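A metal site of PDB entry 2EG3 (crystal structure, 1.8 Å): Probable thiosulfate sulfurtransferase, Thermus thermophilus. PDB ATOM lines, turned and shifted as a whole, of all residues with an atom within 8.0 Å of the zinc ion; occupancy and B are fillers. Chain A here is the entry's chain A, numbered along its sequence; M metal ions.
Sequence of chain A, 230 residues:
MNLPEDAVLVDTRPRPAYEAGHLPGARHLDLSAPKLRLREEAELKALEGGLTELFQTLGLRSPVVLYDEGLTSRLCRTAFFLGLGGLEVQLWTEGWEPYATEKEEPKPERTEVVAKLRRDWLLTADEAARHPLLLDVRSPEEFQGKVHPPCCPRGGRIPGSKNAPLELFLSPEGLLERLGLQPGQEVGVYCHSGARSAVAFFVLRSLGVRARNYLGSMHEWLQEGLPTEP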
ATOM      1  N   LYS A  35     -32.029 -18.167   8.446  1.00  0.00           N
ATOM      2  CA  LYS A  35     -31.059 -17.093   8.667  1.00  0.00           C
ATOM      3  C   LYS A  35     -30.745 -17.158  10.158  1.00  0.00           C
ATOM      4  O   LYS A  35     -31.535 -16.736  11.008  1.00  0.00           O
ATOM      5  CB  LYS A  35     -31.672 -15.750   8.247  1.00  0.00           C
ATOM      6  CG  LYS A  35     -31.757 -15.663   6.735  1.00  0.00           C
ATOM      7  CD  LYS A  35     -32.274 -14.315   6.235  1.00  0.00           C
ATOM      8  CE  LYS A  35     -32.244 -14.266   4.720  1.00  0.00           C
ATOM      9  NZ  LYS A  35     -33.090 -15.363   4.096  1.00  0.00           N
ATOM     10  N   HIS A 148     -25.967  -7.251  -4.516  1.00  0.00           N
ATOM     11  CA  HIS A 148     -26.321  -7.844  -3.235  1.00  0.00           C
ATOM     12  C   HIS A 148     -27.832  -7.964  -3.166  1.00  0.00           C
ATOM     13  O   HIS A 148     -28.558  -7.231  -3.863  1.00  0.00           O
ATOM     14  CB  HIS A 148     -25.859  -6.961  -2.073  1.00  0.00           C
ATOM     15  CG  HIS A 148     -26.605  -5.671  -1.967  1.00  0.00           C
ATOM     16  ND1 HIS A 148     -26.252  -4.545  -2.697  1.00  0.00           N
ATOM     17  CD2 HIS A 148     -27.683  -5.308  -1.222  1.00  0.00           C
ATOM     18  CE1 HIS A 148     -27.080  -3.558  -2.399  1.00  0.00           C
ATOM     19  NE2 HIS A 148     -27.954  -3.994  -1.506  1.00  0.00           N
ATOM     20  N   PRO A 149     -28.334  -8.901  -2.353  1.00  0.00           N
ATOM     21  CA  PRO A 149     -29.784  -9.096  -2.212  1.00  0.00           C
ATOM     22  C   PRO A 149     -30.296  -7.956  -1.328  1.00  0.00           C
ATOM     23  O   PRO A 149     -29.587  -7.457  -0.454  1.00  0.00           O
ATOM     24  CB  PRO A 149     -29.891 -10.477  -1.574  1.00  0.00           C
ATOM     25  CG  PRO A 149     -28.593 -10.592  -0.758  1.00  0.00           C
ATOM     26  CD  PRO A 149     -27.578  -9.996  -1.723  1.00  0.00           C
ATOM     27  N   PRO A 150     -31.552  -7.513  -1.553  1.00  0.00           N
ATOM     28  CA  PRO A 150     -32.183  -6.427  -0.810  1.00  0.00           C
ATOM     29  C   PRO A 150     -32.339  -6.622   0.691  1.00  0.00           C
ATOM     30  O   PRO A 150     -32.657  -5.669   1.405  1.00  0.00           O
ATOM     31  CB  PRO A 150     -33.529  -6.262  -1.532  1.00  0.00           C
ATOM     32  CG  PRO A 150     -33.843  -7.628  -1.957  1.00  0.00           C
ATOM     33  CD  PRO A 150     -32.514  -8.186  -2.432  1.00  0.00           C
ATOM     34  N   CYS A 151     -32.158  -7.850   1.189  1.00  0.00           N
ATOM     35  CA  CYS A 151     -32.243  -8.083   2.628  1.00  0.00           C
ATOM     36  C   CYS A 151     -30.912  -7.710   3.301  1.00  0.00           C
ATOM     37  O   CYS A 151     -30.809  -7.709   4.541  1.00  0.00           O
ATOM     38  CB  CYS A 151     -32.548  -9.549   2.921  1.00  0.00           C
ATOM     39  SG  CYS A 151     -31.363 -10.703   2.108  1.00  0.00           S
ATOM     40  N   CYS A 152     -29.887  -7.431   2.494  1.00  0.00           N
ATOM     41  CA  CYS A 152     -28.566  -7.059   3.008  1.00  0.00           C
ATOM     42  C   CYS A 152     -28.290  -5.595   2.721  1.00  0.00           C
ATOM     43  O   CYS A 152     -28.716  -5.051   1.693  1.00  0.00           O
ATOM     44  CB  CYS A 152     -27.485  -7.941   2.389  1.00  0.00           C
ATOM     45  SG  CYS A 152     -27.388  -9.614   3.157  1.00  0.00           S
ATOM     46  N   PRO A 153     -27.530  -4.929   3.611  1.00  0.00           N
ATOM     47  CA  PRO A 153     -27.225  -3.511   3.435  1.00  0.00           C
ATOM     48  C   PRO A 153     -26.319  -3.056   2.311  1.00  0.00           C
ATOM     49  O   PRO A 153     -26.430  -1.911   1.878  1.00  0.00           O
ATOM     50  CB  PRO A 153     -26.667  -3.107   4.801  1.00  0.00           C
ATOM     51  CG  PRO A 153     -25.986  -4.370   5.263  1.00  0.00           C
ATOM     52  CD  PRO A 153     -26.979  -5.448   4.883  1.00  0.00           C
ATOM     53  N   ARG A 154     -25.425  -3.925   1.847  1.00  0.00           N
ATOM     54  CA  ARG A 154     -24.517  -3.556   0.757  1.00  0.00           C
ATOM     55  C   ARG A 154     -23.885  -4.777   0.133  1.00  0.00           C
ATOM     56  O   ARG A 154     -24.042  -5.912   0.614  1.00  0.00           O
ATOM     57  CB  ARG A 154     -23.403  -2.627   1.290  1.00  0.00           C
ATOM     58  CG  ARG A 154     -22.493  -3.248   2.354  1.00  0.00           C
ATOM     59  CD  ARG A 154     -21.611  -2.165   2.987  1.00  0.00           C
ATOM     60  NE  ARG A 154     -22.437  -1.144   3.642  1.00  0.00           N
ATOM     61  CZ  ARG A 154     -23.003  -1.304   4.848  1.00  0.00           C
ATOM     62  NH1 ARG A 154     -22.811  -2.427   5.530  1.00  0.00           N
ATOM     63  NH2 ARG A 154     -23.780  -0.343   5.350  1.00  0.00           N
ATOM     64  N   HIS A 192     -24.513 -16.582   1.076  1.00  0.00           N
ATOM     65  CA  HIS A 192     -25.363 -15.508   1.619  1.00  0.00           C
ATOM     66  C   HIS A 192     -25.967 -15.860   2.974  1.00  0.00           C
ATOM     67  O   HIS A 192     -25.767 -15.142   3.958  1.00  0.00           O
ATOM     68  CB  HIS A 192     -26.495 -15.165   0.613  1.00  0.00           C
ATOM     69  CG  HIS A 192     -27.545 -14.251   1.176  1.00  0.00           C
ATOM     70  ND1 HIS A 192     -28.884 -14.566   1.157  1.00  0.00           N
ATOM     71  CD2 HIS A 192     -27.453 -13.053   1.809  1.00  0.00           C
ATOM     72  CE1 HIS A 192     -29.570 -13.612   1.748  1.00  0.00           C
ATOM     73  NE2 HIS A 192     -28.729 -12.681   2.153  1.00  0.00           N
ATOM     74  N   SER A 193     -26.682 -16.977   3.035  1.00  0.00           N
ATOM     75  CA  SER A 193     -27.304 -17.366   4.293  1.00  0.00           C
ATOM     76  C   SER A 193     -27.158 -18.851   4.580  1.00  0.00           C
ATOM     77  O   SER A 193     -27.972 -19.433   5.292  1.00  0.00           O
ATOM     78  CB  SER A 193     -28.796 -16.992   4.267  1.00  0.00           C
ATOM     79  OG  SER A 193     -29.439 -17.671   3.200  1.00  0.00           O
ATOM     80  N   GLY A 216     -24.060 -18.669   9.178  1.00  0.00           N
ATOM     81  CA  GLY A 216     -24.508 -17.283   9.254  1.00  0.00           C
ATOM     82  C   GLY A 216     -24.261 -16.575   7.927  1.00  0.00           C
ATOM     83  O   GLY A 216     -25.080 -15.781   7.439  1.00  0.00           O
ATOM     84  N   MET A 218     -22.761 -14.309   4.719  1.00  0.00           N
ATOM     85  CA  MET A 218     -22.726 -12.862   4.533  1.00  0.00           C
ATOM     86  C   MET A 218     -23.855 -12.138   5.217  1.00  0.00           C
ATOM     87  O   MET A 218     -23.670 -11.026   5.741  1.00  0.00           O
ATOM     88  CB  MET A 218     -22.758 -12.456   3.051  1.00  0.00           C
ATOM     89  CG  MET A 218     -21.451 -12.460   2.322  1.00  0.00           C
ATOM     90  SD  MET A 218     -20.033 -11.706   3.201  1.00  0.00           S
ATOM     91  CE  MET A 218     -20.360  -9.990   3.211  1.00  0.00           C
ATOM     92  N   HIS A 219     -25.031 -12.744   5.196  1.00  0.00           N
ATOM     93  CA  HIS A 219     -26.176 -12.071   5.787  1.00  0.00           C
ATOM     94  C   HIS A 219     -25.961 -11.830   7.276  1.00  0.00           C
ATOM     95  O   HIS A 219     -26.190 -10.711   7.751  1.00  0.00           O
ATOM     96  CB  HIS A 219     -27.451 -12.886   5.543  1.00  0.00           C
ATOM     97  CG  HIS A 219     -28.692 -12.216   6.034  1.00  0.00           C
ATOM     98  ND1 HIS A 219     -29.465 -11.397   5.245  1.00  0.00           N
ATOM     99  CD2 HIS A 219     -29.262 -12.192   7.265  1.00  0.00           C
ATOM    100  CE1 HIS A 219     -30.466 -10.907   5.959  1.00  0.00           C
ATOM    101  NE2 HIS A 219     -30.360 -11.366   7.195  1.00  0.00           N
ATOM    102  N   GLU A 220     -25.506 -12.842   8.023  1.00  0.00           N
ATOM    103  CA  GLU A 220     -25.272 -12.573   9.445  1.00  0.00           C
ATOM    104  C   GLU A 220     -24.109 -11.593   9.617  1.00  0.00           C
ATOM    105  O   GLU A 220     -24.184 -10.648  10.424  1.00  0.00           O
ATOM    106  CB  GLU A 220     -24.965 -13.860  10.229  1.00  0.00           C
ATOM    107  CG  GLU A 220     -24.609 -13.528  11.686  1.00  0.00           C
ATOM    108  CD  GLU A 220     -23.998 -14.700  12.427  1.00  0.00           C
ATOM    109  OE1 GLU A 220     -23.176 -15.417  11.827  1.00  0.00           O
ATOM    110  OE2 GLU A 220     -24.326 -14.893  13.618  1.00  0.00           O
ATOM    111  N   LEU A 222     -23.106  -9.187   7.778  1.00  0.00           N
ATOM    112  CA  LEU A 222     -23.535  -7.803   7.576  1.00  0.00           C
ATOM    113  C   LEU A 222     -24.505  -7.325   8.653  1.00  0.00           C
ATOM    114  O   LEU A 222     -24.448  -6.155   9.078  1.00  0.00           O
ATOM    115  CB  LEU A 222     -24.130  -7.626   6.166  1.00  0.00           C
ATOM    116  CG  LEU A 222     -23.093  -7.768   5.043  1.00  0.00           C
ATOM    117  CD1 LEU A 222     -23.806  -7.785   3.676  1.00  0.00           C
ATOM    118  CD2 LEU A 222     -22.081  -6.609   5.101  1.00  0.00           C
ATOM    119  N   GLN A 223     -25.393  -8.203   9.116  1.00  0.00           N
ATOM    120  CA  GLN A 223     -26.320  -7.800  10.169  1.00  0.00           C
ATOM    121  C   GLN A 223     -25.560  -7.424  11.449  1.00  0.00           C
ATOM    122  O   GLN A 223     -25.988  -6.532  12.202  1.00  0.00           O
ATOM    123  CB  GLN A 223     -27.326  -8.912  10.485  1.00  0.00           C
ATOM    124  CG  GLN A 223     -28.410  -9.096   9.427  1.00  0.00           C
ATOM    125  CD  GLN A 223     -29.341  -7.873   9.301  1.00  0.00           C
ATOM    126  OE1 GLN A 223     -29.835  -7.341  10.305  1.00  0.00           O
ATOM    127  NE2 GLN A 223     -29.581  -7.437   8.070  1.00  0.00           N
HETATM  128 ZN    ZN M   1     -29.286 -10.917   3.170  1.00  0.00          ZN
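The zinc ion is bound by NE2 of His 192 (2.1 Å), ND1 of His 219 (2.1 Å), SG of Cys 152 (2.3 Å) and SG of Cys 151 (2.3 Å).
O of His 192 lies within hydrogen-bond range of N of Met 218 (3.2 Å). The backbone carbonyl oxygen of Cys 152 lies close to a ring nitrogen (NE2) of His 148 (3.5 Å).
Four residues have an atom within 4 Å of the zinc ion: Cys 151, Cys 152, His 192 and His 219. Along chain A the residues within 4 Å of the zinc ion span positions 151 to 219.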
